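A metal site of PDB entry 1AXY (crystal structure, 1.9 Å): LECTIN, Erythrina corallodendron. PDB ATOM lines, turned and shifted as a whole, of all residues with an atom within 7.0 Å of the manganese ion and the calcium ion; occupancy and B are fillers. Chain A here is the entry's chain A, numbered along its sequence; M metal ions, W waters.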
ATOM      1  N   ASP A  89      20.810   3.998  27.911  1.00  0.00           N
ATOM      2  CA  ASP A  89      21.342   3.156  26.849  1.00  0.00           C
ATOM      3  C   ASP A  89      21.413   1.676  27.276  1.00  0.00           C
ATOM      4  O   ASP A  89      21.411   0.774  26.413  1.00  0.00           O
ATOM      5  CB  ASP A  89      22.740   3.617  26.456  1.00  0.00           C
ATOM      6  CG  ASP A  89      22.716   4.534  25.246  1.00  0.00           C
ATOM      7  OD1 ASP A  89      22.569   4.029  24.119  1.00  0.00           O
ATOM      8  OD2 ASP A  89      22.848   5.765  25.420  1.00  0.00           O
ATOM      9  N   GLY A  90      21.505   1.438  28.576  1.00  0.00           N
ATOM     10  CA  GLY A  90      21.560   0.080  29.083  1.00  0.00           C
ATOM     11  C   GLY A  90      22.638  -0.140  30.123  1.00  0.00           C
ATOM     12  O   GLY A  90      23.264   0.809  30.574  1.00  0.00           O
ATOM     13  N   TYR A 106      27.069   6.342  26.545  1.00  0.00           N
ATOM     14  CA  TYR A 106      26.002   6.117  25.586  1.00  0.00           C
ATOM     15  C   TYR A 106      25.954   4.644  25.178  1.00  0.00           C
ATOM     16  O   TYR A 106      26.134   3.759  26.017  1.00  0.00           O
ATOM     17  CB  TYR A 106      26.160   7.037  24.362  1.00  0.00           C
ATOM     18  CG  TYR A 106      26.479   8.469  24.736  1.00  0.00           C
ATOM     19  CD1 TYR A 106      25.721   9.142  25.682  1.00  0.00           C
ATOM     20  CD2 TYR A 106      27.565   9.121  24.168  1.00  0.00           C
ATOM     21  CE1 TYR A 106      26.044  10.438  26.067  1.00  0.00           C
ATOM     22  CE2 TYR A 106      27.901  10.401  24.544  1.00  0.00           C
ATOM     23  CZ  TYR A 106      27.135  11.063  25.485  1.00  0.00           C
ATOM     24  OH  TYR A 106      27.457  12.346  25.859  1.00  0.00           O
ATOM     25  N   GLY A 107      25.753   4.407  23.880  1.00  0.00           N
ATOM     26  CA  GLY A 107      25.672   3.055  23.353  1.00  0.00           C
ATOM     27  C   GLY A 107      26.910   2.208  23.531  1.00  0.00           C
ATOM     28  O   GLY A 107      26.867   1.013  23.247  1.00  0.00           O
ATOM     29  N   TYR A 108      28.016   2.819  23.942  1.00  0.00           N
ATOM     30  CA  TYR A 108      29.258   2.057  24.161  1.00  0.00           C
ATOM     31  C   TYR A 108      29.285   1.492  25.570  1.00  0.00           C
ATOM     32  O   TYR A 108      30.210   0.783  25.942  1.00  0.00           O
ATOM     33  CB  TYR A 108      30.482   2.917  23.862  1.00  0.00           C
ATOM     34  CG  TYR A 108      30.506   3.378  22.421  1.00  0.00           C
ATOM     35  CD1 TYR A 108      30.560   2.445  21.378  1.00  0.00           C
ATOM     36  CD2 TYR A 108      30.417   4.720  22.093  1.00  0.00           C
ATOM     37  CE1 TYR A 108      30.528   2.853  20.045  1.00  0.00           C
ATOM     38  CE2 TYR A 108      30.371   5.134  20.773  1.00  0.00           C
ATOM     39  CZ  TYR A 108      30.428   4.196  19.754  1.00  0.00           C
ATOM     40  OH  TYR A 108      30.383   4.624  18.444  1.00  0.00           O
ATOM     41  N   LEU A 109      28.260   1.850  26.344  1.00  0.00           N
ATOM     42  CA  LEU A 109      28.047   1.370  27.701  1.00  0.00           C
ATOM     43  C   LEU A 109      29.161   1.560  28.718  1.00  0.00           C
ATOM     44  O   LEU A 109      29.185   0.888  29.752  1.00  0.00           O
ATOM     45  CB  LEU A 109      27.602  -0.115  27.647  1.00  0.00           C
ATOM     46  CG  LEU A 109      26.396  -0.400  26.750  1.00  0.00           C
ATOM     47  CD1 LEU A 109      26.126  -1.900  26.649  1.00  0.00           C
ATOM     48  CD2 LEU A 109      25.162   0.317  27.268  1.00  0.00           C
ATOM     49  N   GLU A 127      25.633  -7.694  27.888  1.00  0.00           N
ATOM     50  CA  GLU A 127      24.832  -6.483  27.912  1.00  0.00           C
ATOM     51  C   GLU A 127      23.331  -6.678  27.979  1.00  0.00           C
ATOM     52  O   GLU A 127      22.787  -7.715  27.573  1.00  0.00           O
ATOM     53  CB  GLU A 127      25.153  -5.622  26.699  1.00  0.00           C
ATOM     54  CG  GLU A 127      25.084  -6.405  25.399  1.00  0.00           C
ATOM     55  CD  GLU A 127      24.731  -5.559  24.194  1.00  0.00           C
ATOM     56  OE1 GLU A 127      25.529  -4.709  23.753  1.00  0.00           O
ATOM     57  OE2 GLU A 127      23.628  -5.748  23.666  1.00  0.00           O
ATOM     58  N   PHE A 128      22.667  -5.646  28.505  1.00  0.00           N
ATOM     59  CA  PHE A 128      21.225  -5.540  28.633  1.00  0.00           C
ATOM     60  C   PHE A 128      20.991  -4.158  28.014  1.00  0.00           C
ATOM     61  O   PHE A 128      21.005  -3.124  28.676  1.00  0.00           O
ATOM     62  CB  PHE A 128      20.824  -5.655  30.102  1.00  0.00           C
ATOM     63  CG  PHE A 128      21.200  -6.976  30.695  1.00  0.00           C
ATOM     64  CD1 PHE A 128      20.335  -8.075  30.594  1.00  0.00           C
ATOM     65  CD2 PHE A 128      22.461  -7.170  31.249  1.00  0.00           C
ATOM     66  CE1 PHE A 128      20.730  -9.343  31.018  1.00  0.00           C
ATOM     67  CE2 PHE A 128      22.861  -8.433  31.694  1.00  0.00           C
ATOM     68  CZ  PHE A 128      21.992  -9.527  31.569  1.00  0.00           C
ATOM     69  N   ASP A 129      20.948  -4.201  26.688  1.00  0.00           N
ATOM     70  CA  ASP A 129      20.815  -3.048  25.817  1.00  0.00           C
ATOM     71  C   ASP A 129      19.376  -2.585  25.566  1.00  0.00           C
ATOM     72  O   ASP A 129      18.570  -3.301  24.993  1.00  0.00           O
ATOM     73  CB  ASP A 129      21.490  -3.397  24.506  1.00  0.00           C
ATOM     74  CG  ASP A 129      21.816  -2.194  23.679  1.00  0.00           C
ATOM     75  OD1 ASP A 129      21.237  -1.106  23.868  1.00  0.00           O
ATOM     76  OD2 ASP A 129      22.691  -2.325  22.822  1.00  0.00           O
ATOM     77  N   THR A 130      19.125  -1.312  25.886  1.00  0.00           N
ATOM     78  CA  THR A 130      17.795  -0.730  25.753  1.00  0.00           C
ATOM     79  C   THR A 130      17.589   0.233  24.580  1.00  0.00           C
ATOM     80  O   THR A 130      16.464   0.697  24.359  1.00  0.00           O
ATOM     81  CB  THR A 130      17.422   0.030  27.045  1.00  0.00           C
ATOM     82  OG1 THR A 130      18.402   1.043  27.295  1.00  0.00           O
ATOM     83  CG2 THR A 130      17.361  -0.932  28.228  1.00  0.00           C
ATOM     84  N   PHE A 131      18.658   0.556  23.849  1.00  0.00           N
ATOM     85  CA  PHE A 131      18.554   1.472  22.725  1.00  0.00           C
ATOM     86  C   PHE A 131      19.186   0.865  21.480  1.00  0.00           C
ATOM     87  O   PHE A 131      20.296   0.373  21.517  1.00  0.00           O
ATOM     88  CB  PHE A 131      19.236   2.805  23.042  1.00  0.00           C
ATOM     89  CG  PHE A 131      19.187   3.794  21.914  1.00  0.00           C
ATOM     90  CD1 PHE A 131      18.066   4.588  21.706  1.00  0.00           C
ATOM     91  CD2 PHE A 131      20.275   3.938  21.052  1.00  0.00           C
ATOM     92  CE1 PHE A 131      18.010   5.495  20.659  1.00  0.00           C
ATOM     93  CE2 PHE A 131      20.243   4.849  19.999  1.00  0.00           C
ATOM     94  CZ  PHE A 131      19.110   5.628  19.802  1.00  0.00           C
ATOM     95  N   SER A 132      18.480   0.935  20.355  1.00  0.00           N
ATOM     96  CA  SER A 132      18.988   0.363  19.110  1.00  0.00           C
ATOM     97  C   SER A 132      19.906   1.284  18.298  1.00  0.00           C
ATOM     98  O   SER A 132      19.442   2.231  17.664  1.00  0.00           O
ATOM     99  CB  SER A 132      17.824  -0.121  18.252  1.00  0.00           C
ATOM    100  OG  SER A 132      18.286  -0.947  17.197  1.00  0.00           O
ATOM    101  N   ASN A 133      21.208   1.004  18.355  1.00  0.00           N
ATOM    102  CA  ASN A 133      22.228   1.755  17.607  1.00  0.00           C
ATOM    103  C   ASN A 133      22.348   1.101  16.219  1.00  0.00           C
ATOM    104  O   ASN A 133      21.790   0.039  15.975  1.00  0.00           O
ATOM    105  CB  ASN A 133      23.571   1.692  18.340  1.00  0.00           C
ATOM    106  CG  ASN A 133      23.568   2.439  19.654  1.00  0.00           C
ATOM    107  OD1 ASN A 133      23.326   1.868  20.712  1.00  0.00           O
ATOM    108  ND2 ASN A 133      23.858   3.711  19.602  1.00  0.00           N
ATOM    109  N   PRO A 134      23.085   1.739  15.291  1.00  0.00           N
ATOM    110  CA  PRO A 134      23.209   1.143  13.960  1.00  0.00           C
ATOM    111  C   PRO A 134      23.904  -0.202  13.911  1.00  0.00           C
ATOM    112  O   PRO A 134      23.778  -0.922  12.937  1.00  0.00           O
ATOM    113  CB  PRO A 134      23.964   2.219  13.169  1.00  0.00           C
ATOM    114  CG  PRO A 134      24.733   2.933  14.190  1.00  0.00           C
ATOM    115  CD  PRO A 134      23.733   3.053  15.332  1.00  0.00           C
ATOM    116  N   TRP A 135      24.628  -0.548  14.971  1.00  0.00           N
ATOM    117  CA  TRP A 135      25.304  -1.842  15.054  1.00  0.00           C
ATOM    118  C   TRP A 135      24.445  -2.896  15.775  1.00  0.00           C
ATOM    119  O   TRP A 135      24.836  -4.061  15.895  1.00  0.00           O
ATOM    120  CB  TRP A 135      26.648  -1.700  15.764  1.00  0.00           C
ATOM    121  CG  TRP A 135      26.528  -1.105  17.132  1.00  0.00           C
ATOM    122  CD1 TRP A 135      26.102  -1.735  18.265  1.00  0.00           C
ATOM    123  CD2 TRP A 135      26.851   0.232  17.513  1.00  0.00           C
ATOM    124  NE1 TRP A 135      26.135  -0.874  19.334  1.00  0.00           N
ATOM    125  CE2 TRP A 135      26.603   0.339  18.901  1.00  0.00           C
ATOM    126  CE3 TRP A 135      27.336   1.347  16.823  1.00  0.00           C
ATOM    127  CZ2 TRP A 135      26.819   1.526  19.609  1.00  0.00           C
ATOM    128  CZ3 TRP A 135      27.550   2.525  17.533  1.00  0.00           C
ATOM    129  CH2 TRP A 135      27.291   2.599  18.908  1.00  0.00           C
ATOM    130  N   ASP A 136      23.267  -2.485  16.224  1.00  0.00           N
ATOM    131  CA  ASP A 136      22.337  -3.356  16.946  1.00  0.00           C
ATOM    132  C   ASP A 136      21.226  -3.937  16.119  1.00  0.00           C
ATOM    133  O   ASP A 136      20.878  -3.412  15.054  1.00  0.00           O
ATOM    134  CB  ASP A 136      21.630  -2.557  18.034  1.00  0.00           C
ATOM    135  CG  ASP A 136      22.493  -2.304  19.211  1.00  0.00           C
ATOM    136  OD1 ASP A 136      23.304  -3.179  19.517  1.00  0.00           O
ATOM    137  OD2 ASP A 136      22.381  -1.236  19.835  1.00  0.00           O
ATOM    138  N   PRO A 137      20.648  -5.056  16.585  1.00  0.00           N
ATOM    139  CA  PRO A 137      19.531  -5.663  15.847  1.00  0.00           C
ATOM    140  C   PRO A 137      18.402  -4.662  16.131  1.00  0.00           C
ATOM    141  O   PRO A 137      18.493  -3.870  17.075  1.00  0.00           O
ATOM    142  CB  PRO A 137      19.316  -6.985  16.589  1.00  0.00           C
ATOM    143  CG  PRO A 137      19.858  -6.727  17.971  1.00  0.00           C
ATOM    144  CD  PRO A 137      21.114  -5.938  17.665  1.00  0.00           C
ATOM    145  N   VAL A 140      14.725  -4.111  20.795  1.00  0.00           N
ATOM    146  CA  VAL A 140      15.253  -3.685  22.090  1.00  0.00           C
ATOM    147  C   VAL A 140      14.097  -3.781  23.074  1.00  0.00           C
ATOM    148  O   VAL A 140      12.943  -3.576  22.706  1.00  0.00           O
ATOM    149  CB  VAL A 140      15.828  -2.232  22.086  1.00  0.00           C
ATOM    150  CG1 VAL A 140      17.193  -2.195  21.448  1.00  0.00           C
ATOM    151  CG2 VAL A 140      14.882  -1.289  21.371  1.00  0.00           C
ATOM    152  N   HIS A 142      17.517  -6.053  24.494  1.00  0.00           N
ATOM    153  CA  HIS A 142      18.102  -7.349  24.175  1.00  0.00           C
ATOM    154  C   HIS A 142      19.325  -7.644  25.015  1.00  0.00           C
ATOM    155  O   HIS A 142      20.000  -6.729  25.493  1.00  0.00           O
ATOM    156  CB  HIS A 142      18.440  -7.493  22.683  1.00  0.00           C
ATOM    157  CG  HIS A 142      19.415  -6.485  22.174  1.00  0.00           C
ATOM    158  ND1 HIS A 142      19.054  -5.339  21.493  1.00  0.00           N
ATOM    159  CD2 HIS A 142      20.774  -6.453  22.252  1.00  0.00           C
ATOM    160  CE1 HIS A 142      20.168  -4.669  21.194  1.00  0.00           C
ATOM    161  NE2 HIS A 142      21.236  -5.303  21.632  1.00  0.00           N
ATOM    162  N   ILE A 143      19.532  -8.923  25.270  1.00  0.00           N
ATOM    163  CA  ILE A 143      20.695  -9.387  25.995  1.00  0.00           C
ATOM    164  C   ILE A 143      21.725  -9.639  24.894  1.00  0.00           C
ATOM    165  O   ILE A 143      21.364 -10.076  23.788  1.00  0.00           O
ATOM    166  CB  ILE A 143      20.435 -10.747  26.688  1.00  0.00           C
ATOM    167  CG1 ILE A 143      19.166 -10.685  27.553  1.00  0.00           C
ATOM    168  CG2 ILE A 143      21.633 -11.137  27.547  1.00  0.00           C
ATOM    169  CD1 ILE A 143      18.711 -12.030  28.054  1.00  0.00           C
ATOM    170  N   GLY A 144      22.978  -9.326  25.143  1.00  0.00           N
ATOM    171  CA  GLY A 144      23.979  -9.581  24.122  1.00  0.00           C
ATOM    172  C   GLY A 144      25.295 -10.016  24.720  1.00  0.00           C
ATOM    173  O   GLY A 144      25.626  -9.625  25.831  1.00  0.00           O
ATOM    174  N   ASP A 146      29.120  -9.718  24.271  1.00  0.00           N
ATOM    175  CA  ASP A 146      30.118  -8.873  23.612  1.00  0.00           C
ATOM    176  C   ASP A 146      31.524  -9.404  23.792  1.00  0.00           C
ATOM    177  O   ASP A 146      31.981  -9.595  24.912  1.00  0.00           O
ATOM    178  CB  ASP A 146      30.051  -7.442  24.167  1.00  0.00           C
ATOM    179  CG  ASP A 146      28.672  -6.809  24.031  1.00  0.00           C
ATOM    180  OD1 ASP A 146      27.828  -7.368  23.314  1.00  0.00           O
ATOM    181  OD2 ASP A 146      28.425  -5.767  24.656  1.00  0.00           O
ATOM    182  N   ILE A 150      31.311  -3.850  20.752  1.00  0.00           N
ATOM    183  CA  ILE A 150      29.951  -3.549  21.173  1.00  0.00           C
ATOM    184  C   ILE A 150      28.965  -4.273  20.224  1.00  0.00           C
ATOM    185  O   ILE A 150      27.770  -4.362  20.503  1.00  0.00           O
ATOM    186  CB  ILE A 150      29.711  -2.002  21.198  1.00  0.00           C
ATOM    187  CG1 ILE A 150      28.400  -1.666  21.921  1.00  0.00           C
ATOM    188  CG2 ILE A 150      29.761  -1.411  19.785  1.00  0.00           C
ATOM    189  CD1 ILE A 150      28.405  -2.015  23.405  1.00  0.00           C
ATOM    190  N   ARG A 151      29.477  -4.786  19.116  1.00  0.00           N
ATOM    191  CA  ARG A 151      28.668  -5.540  18.149  1.00  0.00           C
ATOM    192  C   ARG A 151      28.624  -6.976  18.645  1.00  0.00           C
ATOM    193  O   ARG A 151      29.522  -7.769  18.340  1.00  0.00           O
ATOM    194  CB  ARG A 151      29.324  -5.522  16.773  1.00  0.00           C
ATOM    195  CG  ARG A 151      29.608  -4.166  16.193  1.00  0.00           C
ATOM    196  CD  ARG A 151      29.966  -4.335  14.740  1.00  0.00           C
ATOM    197  NE  ARG A 151      31.291  -3.821  14.445  1.00  0.00           N
ATOM    198  CZ  ARG A 151      32.262  -4.520  13.850  1.00  0.00           C
ATOM    199  NH1 ARG A 151      32.068  -5.777  13.467  1.00  0.00           N
ATOM    200  NH2 ARG A 151      33.400  -3.914  13.563  1.00  0.00           N
ATOM    201  N   SER A 152      27.564  -7.334  19.372  1.00  0.00           N
ATOM    202  CA  SER A 152      27.420  -8.676  19.946  1.00  0.00           C
ATOM    203  C   SER A 152      27.578  -9.816  18.955  1.00  0.00           C
ATOM    204  O   SER A 152      27.191  -9.698  17.809  1.00  0.00           O
ATOM    205  CB  SER A 152      26.055  -8.823  20.610  1.00  0.00           C
ATOM    206  OG  SER A 152      25.805  -7.716  21.459  1.00  0.00           O
ATOM    207  N   THR A 155      22.699 -12.300  20.184  1.00  0.00           N
ATOM    208  CA  THR A 155      21.721 -11.417  20.791  1.00  0.00           C
ATOM    209  C   THR A 155      20.420 -12.163  21.104  1.00  0.00           C
ATOM    210  O   THR A 155      20.092 -13.134  20.445  1.00  0.00           O
ATOM    211  CB  THR A 155      21.462 -10.214  19.825  1.00  0.00           C
ATOM    212  OG1 THR A 155      22.084  -9.032  20.347  1.00  0.00           O
ATOM    213  CG2 THR A 155      20.007  -9.966  19.586  1.00  0.00           C
HETATM  214 MN    MN M   1      23.467  -4.275  21.642  1.00  0.00          MN
HETATM  215 CA    CA M   2      22.641  -0.094  21.931  1.00  0.00          CA
HETATM  216  O   HOH W   1      25.026  -0.622  22.195  1.00  0.00           O
HETATM  217  O   HOH W   2      24.100  -6.136  20.230  1.00  0.00           O
HETATM  218  O   HOH W   3      25.747  -3.298  21.656  1.00  0.00           O
HETATM  219  O   HOH W   4      22.595   1.390  23.830  1.00  0.00           O
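Four residues have an atom within 4 Å of the calcium ion: Asp 129, Phe 131, Asn 133 and Asp 136.
The nearest printed residue that does not touch the calcium ion is Trp 135 (4.4 Å).
The manganese ion is bound by OD1 of Asp 136 (2.4 Å), OD2 of Asp 129 (2.4 Å), water W2 (2.4 Å), NE2 of His 142 (2.5 Å), water W3 (2.5 Å) and OE2 of Glu 127 (2.5 Å).
The manganese ion has six donor atoms within binding distance.
O of Gly 144 is in hydrogen-bond range of N of Glu 127 (2.8 Å).
Water W3 lies within hydrogen-bond range of the side-chain carboxylate (OE1) of Glu 127, the backbone carbonyl oxygen (O) of Ile 150 and the indole nitrogen (NE1) of Trp 135.
Water W1 bridges the backbone carbonyl oxygen of Gly 107 (2.7 Å) and the indole nitrogen of Trp 135 (3.1 Å).
The calcium ion is bound by the side-chain carboxylate (OD2) of Asp 136 (2.4 Å), the side-chain carboxylate (OD2) of Asp 129 (2.4 Å), the side-chain amide oxygen (OD1) of Asn 133 (2.4 Å), water W4 (2.4 Å), the backbone carbonyl oxygen (O) of Phe 131 (2.4 Å), water W1 (2.5 Å) and the side-chain carboxylate (OD1) of Asp 129 (2.6 Å).
The calcium ion has seven donor atoms within binding distance.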
